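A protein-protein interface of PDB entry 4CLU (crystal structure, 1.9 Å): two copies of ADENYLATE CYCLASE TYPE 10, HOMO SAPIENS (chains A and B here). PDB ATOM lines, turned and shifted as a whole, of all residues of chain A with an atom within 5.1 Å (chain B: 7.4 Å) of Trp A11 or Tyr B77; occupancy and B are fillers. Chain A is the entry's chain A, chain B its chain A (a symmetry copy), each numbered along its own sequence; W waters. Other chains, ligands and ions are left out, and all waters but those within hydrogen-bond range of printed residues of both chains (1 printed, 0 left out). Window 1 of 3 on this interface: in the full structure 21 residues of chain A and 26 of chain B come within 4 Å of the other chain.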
ATOM      1  N   GLN A   9      21.241  31.922  15.020  1.00  0.00           N
ATOM      2  CA  GLN A   9      21.852  32.160  16.301  1.00  0.00           C
ATOM      3  C   GLN A   9      23.076  33.118  16.145  1.00  0.00           C
ATOM      4  O   GLN A   9      24.112  32.781  15.505  1.00  0.00           O
ATOM      5  CB  GLN A   9      22.167  30.823  16.994  1.00  0.00           C
ATOM      6  CG  GLN A   9      20.996  30.258  17.808  1.00  0.00           C
ATOM      7  CD  GLN A   9      20.663  31.086  19.059  1.00  0.00           C
ATOM      8  OE1 GLN A   9      19.941  30.610  19.934  1.00  0.00           O
ATOM      9  NE2 GLN A   9      21.200  32.311  19.159  1.00  0.00           N
ATOM     10  N   ASP A  10      22.918  34.318  16.710  1.00  0.00           N
ATOM     11  CA  ASP A  10      23.912  35.345  16.577  1.00  0.00           C
ATOM     12  C   ASP A  10      24.808  35.243  17.789  1.00  0.00           C
ATOM     13  O   ASP A  10      24.917  36.168  18.570  1.00  0.00           O
ATOM     14  CB  ASP A  10      23.249  36.718  16.446  1.00  0.00           C
ATOM     15  CG  ASP A  10      24.209  37.773  15.944  1.00  0.00           C
ATOM     16  OD1 ASP A  10      25.098  37.465  15.082  1.00  0.00           O
ATOM     17  OD2 ASP A  10      24.071  38.903  16.425  1.00  0.00           O
ATOM     18  N   TRP A  11      25.467  34.103  17.909  1.00  0.00           N
ATOM     19  CA  TRP A  11      26.438  33.921  18.976  1.00  0.00           C
ATOM     20  C   TRP A  11      27.531  34.977  18.963  1.00  0.00           C
ATOM     21  O   TRP A  11      27.833  35.519  17.889  1.00  0.00           O
ATOM     22  CB  TRP A  11      27.101  32.583  18.803  1.00  0.00           C
ATOM     23  CG  TRP A  11      26.182  31.407  18.829  1.00  0.00           C
ATOM     24  CD1 TRP A  11      25.895  30.617  17.780  1.00  0.00           C
ATOM     25  CD2 TRP A  11      25.524  30.839  19.970  1.00  0.00           C
ATOM     26  NE1 TRP A  11      25.037  29.609  18.191  1.00  0.00           N
ATOM     27  CE2 TRP A  11      24.813  29.729  19.535  1.00  0.00           C
ATOM     28  CE3 TRP A  11      25.430  31.207  21.291  1.00  0.00           C
ATOM     29  CZ2 TRP A  11      24.011  28.933  20.401  1.00  0.00           C
ATOM     30  CZ3 TRP A  11      24.681  30.409  22.187  1.00  0.00           C
ATOM     31  CH2 TRP A  11      23.916  29.324  21.703  1.00  0.00           C
ATOM     32  N   PRO A  12      28.173  35.204  20.117  1.00  0.00           N
ATOM     33  CA  PRO A  12      29.261  36.123  20.168  1.00  0.00           C
ATOM     34  C   PRO A  12      30.366  35.819  19.149  1.00  0.00           C
ATOM     35  O   PRO A  12      30.901  36.728  18.527  1.00  0.00           O
ATOM     36  CB  PRO A  12      29.784  35.978  21.584  1.00  0.00           C
ATOM     37  CG  PRO A  12      28.577  35.576  22.400  1.00  0.00           C
ATOM     38  CD  PRO A  12      27.739  34.771  21.465  1.00  0.00           C
ATOM     39  N   ILE A  13      30.679  34.567  18.936  1.00  0.00           N
ATOM     40  CA  ILE A  13      31.695  34.245  17.927  1.00  0.00           C
ATOM     41  C   ILE A  13      31.336  34.719  16.514  1.00  0.00           C
ATOM     42  O   ILE A  13      32.228  35.176  15.762  1.00  0.00           O
ATOM     43  CB  ILE A  13      32.123  32.769  17.945  1.00  0.00           C
ATOM     44  CG1 ILE A  13      33.491  32.560  17.317  1.00  0.00           C
ATOM     45  CG2 ILE A  13      31.062  31.834  17.344  1.00  0.00           C
ATOM     46  CD1 ILE A  13      33.979  31.098  17.495  1.00  0.00           C
ATOM     47  N   VAL A  14      30.076  34.636  16.151  1.00  0.00           N
ATOM     48  CA  VAL A  14      29.612  35.122  14.863  1.00  0.00           C
ATOM     49  C   VAL A  14      29.727  36.637  14.797  1.00  0.00           C
ATOM     50  O   VAL A  14      30.200  37.210  13.823  1.00  0.00           O
ATOM     51  CB  VAL A  14      28.164  34.632  14.620  1.00  0.00           C
ATOM     52  CG1 VAL A  14      27.558  35.300  13.422  1.00  0.00           C
ATOM     53  CG2 VAL A  14      28.125  33.109  14.511  1.00  0.00           C
ATOM     54  N   ARG A  15      29.364  37.308  15.875  1.00  0.00           N
ATOM     55  CA  ARG A  15      29.464  38.774  15.910  1.00  0.00           C
ATOM     56  C   ARG A  15      30.927  39.245  15.786  1.00  0.00           C
ATOM     57  O   ARG A  15      31.229  40.240  15.111  1.00  0.00           O
ATOM     58  CB  ARG A  15      28.829  39.294  17.209  1.00  0.00           C
ATOM     59  CG  ARG A  15      27.335  39.046  17.351  1.00  0.00           C
ATOM     60  CD  ARG A  15      26.896  39.674  18.725  1.00  0.00           C
ATOM     61  NE  ARG A  15      25.474  39.834  18.733  1.00  0.00           N
ATOM     62  CZ  ARG A  15      24.801  40.658  19.548  1.00  0.00           C
ATOM     63  NH1 ARG A  15      25.430  41.398  20.473  1.00  0.00           N
ATOM     64  NH2 ARG A  15      23.477  40.752  19.398  1.00  0.00           N
ATOM     65  N   LEU A 255      29.356  30.055  11.811  1.00  0.00           N
ATOM     66  CA  LEU A 255      30.349  29.610  12.784  1.00  0.00           C
ATOM     67  C   LEU A 255      29.699  29.239  14.105  1.00  0.00           C
ATOM     68  O   LEU A 255      28.739  29.867  14.526  1.00  0.00           O
ATOM     69  CB  LEU A 255      31.322  30.745  13.098  1.00  0.00           C
ATOM     70  CG  LEU A 255      32.529  31.099  12.329  1.00  0.00           C
ATOM     71  CD1 LEU A 255      33.279  32.200  13.124  1.00  0.00           C
ATOM     72  CD2 LEU A 255      33.447  29.918  12.121  1.00  0.00           C
ATOM     73  N   LYS A 256      30.221  28.200  14.728  1.00  0.00           N
ATOM     74  CA  LYS A 256      29.618  27.679  15.929  1.00  0.00           C
ATOM     75  C   LYS A 256      30.561  28.019  17.094  1.00  0.00           C
ATOM     76  O   LYS A 256      31.779  28.135  16.913  1.00  0.00           O
ATOM     77  CB  LYS A 256      29.340  26.182  15.854  1.00  0.00           C
ATOM     78  CG  LYS A 256      28.286  25.833  14.782  1.00  0.00           C
ATOM     79  CD  LYS A 256      27.067  26.746  14.852  1.00  0.00           C
ATOM     80  CE  LYS A 256      26.026  26.240  13.862  1.00  0.00           C
ATOM     81  NZ  LYS A 256      25.114  27.307  13.436  1.00  0.00           N
ATOM     82  N   PRO A 257      29.996  28.203  18.274  1.00  0.00           N
ATOM     83  CA  PRO A 257      30.823  28.368  19.455  1.00  0.00           C
ATOM     84  C   PRO A 257      31.986  27.409  19.553  1.00  0.00           C
ATOM     85  O   PRO A 257      31.824  26.247  19.313  1.00  0.00           O
ATOM     86  CB  PRO A 257      29.846  28.154  20.583  1.00  0.00           C
ATOM     87  CG  PRO A 257      28.645  28.812  20.032  1.00  0.00           C
ATOM     88  CD  PRO A 257      28.581  28.234  18.658  1.00  0.00           C
ATOM     89  N   PHE B  51      31.156  20.958  33.251  1.00  0.00           N
ATOM     90  CA  PHE B  51      31.160  22.383  33.194  1.00  0.00           C
ATOM     91  C   PHE B  51      31.609  22.950  34.459  1.00  0.00           C
ATOM     92  O   PHE B  51      32.100  24.089  34.454  1.00  0.00           O
ATOM     93  CB  PHE B  51      29.840  23.017  32.802  1.00  0.00           C
ATOM     94  CG  PHE B  51      29.772  23.237  31.368  1.00  0.00           C
ATOM     95  CD1 PHE B  51      30.354  24.371  30.810  1.00  0.00           C
ATOM     96  CD2 PHE B  51      29.219  22.258  30.539  1.00  0.00           C
ATOM     97  CE1 PHE B  51      30.339  24.542  29.442  1.00  0.00           C
ATOM     98  CE2 PHE B  51      29.200  22.423  29.144  1.00  0.00           C
ATOM     99  CZ  PHE B  51      29.759  23.573  28.597  1.00  0.00           C
ATOM    100  N   LEU B  71      31.875  31.256  28.564  1.00  0.00           N
ATOM    101  CA  LEU B  71      31.294  30.126  29.287  1.00  0.00           C
ATOM    102  C   LEU B  71      29.837  29.966  28.912  1.00  0.00           C
ATOM    103  O   LEU B  71      29.372  28.859  28.534  1.00  0.00           O
ATOM    104  CB  LEU B  71      31.469  30.358  30.789  1.00  0.00           C
ATOM    105  CG  LEU B  71      30.962  29.259  31.721  1.00  0.00           C
ATOM    106  CD1 LEU B  71      31.680  27.942  31.407  1.00  0.00           C
ATOM    107  CD2 LEU B  71      31.171  29.680  33.180  1.00  0.00           C
ATOM    108  N   VAL B  72      29.098  31.052  28.991  1.00  0.00           N
ATOM    109  CA  VAL B  72      27.699  30.983  28.710  1.00  0.00           C
ATOM    110  C   VAL B  72      27.385  30.636  27.304  1.00  0.00           C
ATOM    111  O   VAL B  72      26.418  29.912  27.075  1.00  0.00           O
ATOM    112  CB  VAL B  72      26.901  32.200  29.206  1.00  0.00           C
ATOM    113  CG1 VAL B  72      27.046  33.435  28.351  1.00  0.00           C
ATOM    114  CG2 VAL B  72      25.438  31.785  29.393  1.00  0.00           C
ATOM    115  N   GLU B  73      28.198  31.134  26.374  1.00  0.00           N
ATOM    116  CA  GLU B  73      28.009  30.830  24.977  1.00  0.00           C
ATOM    117  C   GLU B  73      28.186  29.308  24.722  1.00  0.00           C
ATOM    118  O   GLU B  73      27.342  28.682  24.090  1.00  0.00           O
ATOM    119  CB  GLU B  73      29.052  31.625  24.197  1.00  0.00           C
ATOM    120  CG  GLU B  73      29.012  31.361  22.730  1.00  0.00           C
ATOM    121  CD  GLU B  73      30.030  32.237  21.974  1.00  0.00           C
ATOM    122  OE1 GLU B  73      30.981  32.724  22.640  1.00  0.00           O
ATOM    123  OE2 GLU B  73      29.890  32.321  20.745  1.00  0.00           O
ATOM    124  N   ILE B  74      29.286  28.750  25.203  1.00  0.00           N
ATOM    125  CA  ILE B  74      29.566  27.309  24.954  1.00  0.00           C
ATOM    126  C   ILE B  74      28.580  26.465  25.714  1.00  0.00           C
ATOM    127  O   ILE B  74      28.098  25.486  25.180  1.00  0.00           O
ATOM    128  CB  ILE B  74      31.021  26.887  25.164  1.00  0.00           C
ATOM    129  CG1 ILE B  74      31.329  25.511  24.524  1.00  0.00           C
ATOM    130  CG2 ILE B  74      31.438  26.879  26.615  1.00  0.00           C
ATOM    131  CD1 ILE B  74      31.136  25.409  23.012  1.00  0.00           C
ATOM    132  N   LEU B  75      28.253  26.857  26.931  1.00  0.00           N
ATOM    133  CA  LEU B  75      27.229  26.081  27.694  1.00  0.00           C
ATOM    134  C   LEU B  75      25.904  26.083  26.976  1.00  0.00           C
ATOM    135  O   LEU B  75      25.337  25.023  26.703  1.00  0.00           O
ATOM    136  CB  LEU B  75      27.123  26.671  29.071  1.00  0.00           C
ATOM    137  CG  LEU B  75      26.079  25.942  29.883  1.00  0.00           C
ATOM    138  CD1 LEU B  75      26.433  24.470  29.992  1.00  0.00           C
ATOM    139  CD2 LEU B  75      25.911  26.544  31.222  1.00  0.00           C
ATOM    140  N   ASN B  76      25.411  27.278  26.609  1.00  0.00           N
ATOM    141  CA  ASN B  76      24.132  27.333  25.965  1.00  0.00           C
ATOM    142  C   ASN B  76      24.050  26.721  24.598  1.00  0.00           C
ATOM    143  O   ASN B  76      22.974  26.187  24.184  1.00  0.00           O
ATOM    144  CB  ASN B  76      23.581  28.712  25.960  1.00  0.00           C
ATOM    145  CG  ASN B  76      23.036  29.113  27.331  1.00  0.00           C
ATOM    146  OD1 ASN B  76      22.799  28.268  28.143  1.00  0.00           O
ATOM    147  ND2 ASN B  76      22.841  30.381  27.566  1.00  0.00           N
ATOM    148  N   TYR B  77      25.165  26.738  23.898  1.00  0.00           N
ATOM    149  CA  TYR B  77      25.218  26.043  22.610  1.00  0.00           C
ATOM    150  C   TYR B  77      24.853  24.577  22.792  1.00  0.00           C
ATOM    151  O   TYR B  77      24.043  24.032  22.039  1.00  0.00           O
ATOM    152  CB  TYR B  77      26.591  26.184  22.012  1.00  0.00           C
ATOM    153  CG  TYR B  77      26.789  25.483  20.686  1.00  0.00           C
ATOM    154  CD1 TYR B  77      25.900  25.670  19.643  1.00  0.00           C
ATOM    155  CD2 TYR B  77      27.836  24.588  20.515  1.00  0.00           C
ATOM    156  CE1 TYR B  77      26.092  25.021  18.433  1.00  0.00           C
ATOM    157  CE2 TYR B  77      28.023  23.939  19.296  1.00  0.00           C
ATOM    158  CZ  TYR B  77      27.123  24.160  18.282  1.00  0.00           C
ATOM    159  OH  TYR B  77      27.298  23.519  17.090  1.00  0.00           O
ATOM    160  N   HIS B  78      25.444  23.966  23.799  1.00  0.00           N
ATOM    161  CA  HIS B  78      25.184  22.554  24.107  1.00  0.00           C
ATOM    162  C   HIS B  78      23.815  22.351  24.762  1.00  0.00           C
ATOM    163  O   HIS B  78      23.054  21.499  24.308  1.00  0.00           O
ATOM    164  CB  HIS B  78      26.267  22.028  25.032  1.00  0.00           C
ATOM    165  CG  HIS B  78      27.585  21.937  24.367  1.00  0.00           C
ATOM    166  ND1 HIS B  78      27.895  20.926  23.486  1.00  0.00           N
ATOM    167  CD2 HIS B  78      28.632  22.780  24.348  1.00  0.00           C
ATOM    168  CE1 HIS B  78      29.106  21.128  22.992  1.00  0.00           C
ATOM    169  NE2 HIS B  78      29.573  22.241  23.503  1.00  0.00           N
ATOM    170  N   ILE B  79      23.498  23.087  25.828  1.00  0.00           N
ATOM    171  CA  ILE B  79      22.205  22.916  26.483  1.00  0.00           C
ATOM    172  C   ILE B  79      21.017  23.211  25.589  1.00  0.00           C
ATOM    173  O   ILE B  79      19.976  22.506  25.674  1.00  0.00           O
ATOM    174  CB  ILE B  79      22.151  23.757  27.729  1.00  0.00           C
ATOM    175  CG1 ILE B  79      23.116  23.074  28.700  1.00  0.00           C
ATOM    176  CG2 ILE B  79      20.725  23.819  28.331  1.00  0.00           C
ATOM    177  CD1 ILE B  79      23.405  23.922  29.898  1.00  0.00           C
ATOM    178  N   SER B  80      21.124  24.249  24.730  1.00  0.00           N
ATOM    179  CA  SER B  80      20.063  24.512  23.742  1.00  0.00           C
ATOM    180  C   SER B  80      19.662  23.338  22.884  1.00  0.00           C
ATOM    181  O   SER B  80      18.471  23.153  22.576  1.00  0.00           O
ATOM    182  CB  SER B  80      20.491  25.647  22.757  1.00  0.00           C
ATOM    183  OG  SER B  80      20.349  26.742  23.486  1.00  0.00           O
ATOM    184  N   ALA B  81      20.648  22.588  22.393  1.00  0.00           N
ATOM    185  CA  ALA B  81      20.407  21.434  21.598  1.00  0.00           C
ATOM    186  C   ALA B  81      19.687  20.324  22.386  1.00  0.00           C
ATOM    187  O   ALA B  81      18.768  19.697  21.813  1.00  0.00           O
ATOM    188  CB  ALA B  81      21.726  20.886  20.971  1.00  0.00           C
ATOM    189  N   ILE B  82      20.022  20.168  23.662  1.00  0.00           N
ATOM    190  CA  ILE B  82      19.332  19.202  24.529  1.00  0.00           C
ATOM    191  C   ILE B  82      17.889  19.659  24.810  1.00  0.00           C
ATOM    192  O   ILE B  82      16.948  18.849  24.717  1.00  0.00           O
ATOM    193  CB  ILE B  82      20.040  19.014  25.871  1.00  0.00           C
ATOM    194  CG1 ILE B  82      21.423  18.414  25.707  1.00  0.00           C
ATOM    195  CG2 ILE B  82      19.225  18.145  26.820  1.00  0.00           C
ATOM    196  CD1 ILE B  82      22.188  18.394  27.000  1.00  0.00           C
ATOM    197  N   PHE B 130      26.399  14.288  21.579  1.00  0.00           N
ATOM    198  CA  PHE B 130      27.764  14.658  22.001  1.00  0.00           C
ATOM    199  C   PHE B 130      28.827  13.525  22.022  1.00  0.00           C
ATOM    200  O   PHE B 130      29.065  12.867  23.044  1.00  0.00           O
ATOM    201  CB  PHE B 130      27.703  15.473  23.315  1.00  0.00           C
ATOM    202  CG  PHE B 130      26.803  16.703  23.216  1.00  0.00           C
ATOM    203  CD1 PHE B 130      26.852  17.550  22.076  1.00  0.00           C
ATOM    204  CD2 PHE B 130      25.899  17.011  24.231  1.00  0.00           C
ATOM    205  CE1 PHE B 130      26.014  18.658  21.969  1.00  0.00           C
ATOM    206  CE2 PHE B 130      25.069  18.123  24.127  1.00  0.00           C
ATOM    207  CZ  PHE B 130      25.120  18.943  22.998  1.00  0.00           C
ATOM    208  N   GLY B 397      20.114  27.813  29.064  1.00  0.00           N
ATOM    209  CA  GLY B 397      19.086  27.160  28.340  1.00  0.00           C
ATOM    210  C   GLY B 397      18.973  27.674  26.924  1.00  0.00           C
ATOM    211  O   GLY B 397      19.948  28.140  26.328  1.00  0.00           O
ATOM    212  N   THR B 399      16.663  29.932  23.980  1.00  0.00           N
ATOM    213  CA  THR B 399      15.847  31.147  23.849  1.00  0.00           C
ATOM    214  C   THR B 399      14.403  30.944  24.366  1.00  0.00           C
ATOM    215  O   THR B 399      13.858  31.812  25.035  1.00  0.00           O
ATOM    216  CB  THR B 399      15.736  31.554  22.353  1.00  0.00           C
ATOM    217  OG1 THR B 399      17.031  31.850  21.887  1.00  0.00           O
ATOM    218  CG2 THR B 399      14.888  32.800  22.170  1.00  0.00           C
HETATM  219  O   HOH W   1      18.915  29.173  22.120  1.00  0.00           O
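Printed residues of chain B that touch a printed residue of chain A: Glu B73, Ile B74, Asn B76, Tyr B77 and Thr B399.
Hydrophobic or aromatic side chains of chain B that line the printed part of chain A: Ile B74 and Tyr B77.
Hydrophobic or aromatic side chains of chain A within 4 Å of the printed part of chain B: Trp A11, Pro A12, Ile A13 and Pro A257.
Among the printed residues, 10 pairs touch across the chains.
Among the printed residues, no Asp or Glu carboxylate lies within 4 Å of a Lys or Arg side-chain nitrogen of the other chain.
Water W1 lies within hydrogen-bond range of the side-chain amide oxygen of Gln A9 (2.8 Å), the backbone NH of Thr B399 (3.0 Å) and the side-chain hydroxyl of Ser B80 (3.1 Å).
Of chain B, only Glu B73, Asn B76 and Tyr B77 come within 4 Å of Trp A11.
Of chain A, only Trp A11 (3.6 Å), Lys A256 (3.4 Å) and Pro A257 (3.8 Å) come within 4 Å of Tyr B77.
Printed residues of chain B within 4 Å of Gln A9: Thr B399 (3.7 Å).
Of the printed residues of chain B, Ile A13 touches Glu B73 (3.0 Å).
Of the printed residues of chain B, Pro A12 touches Glu B73 (3.3 Å).
Asp A10 touches none of the printed residues of chain B.
The nearest residue of chain B that does not touch Trp A11 is Ser B80 (4.8 Å).
Among the printed residues, merely in contact across the chains: Gln A9 with Thr B399 (3.7 Å), Trp A11 with Glu B73 (3.4 Å), Trp A11 with Asn B76 (3.9 Å), Trp A11 with Tyr B77 (3.6 Å), Lys A256 with Tyr B77 (3.4 Å), Pro A257 with Glu B73 (3.7 Å), Pro A257 with Ile B74 (3.9 Å) and Pro A257 with Tyr B77 (3.8 Å).
No position is printed for both chains.
Of the 10 pairs that touch across the chains among the printed residues, none has its exchanged pair printed and touching as well.
The backbone NH of Ile A13 lies within hydrogen-bond range of the side-chain carboxylate of Glu B73 (3.0 Å).
The backbone nitrogen of Pro A12 sits close to the side-chain carboxylate of Glu B73, at 3.4 Å.
The side-chain hydroxyl (OG) of Ser B80 lies within hydrogen-bond range of the backbone carbonyl oxygen (O) of Asn B76 (2.8 Å).
N of Gly B397 is in hydrogen-bond range of OD1 of Asn B76 (2.9 Å).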
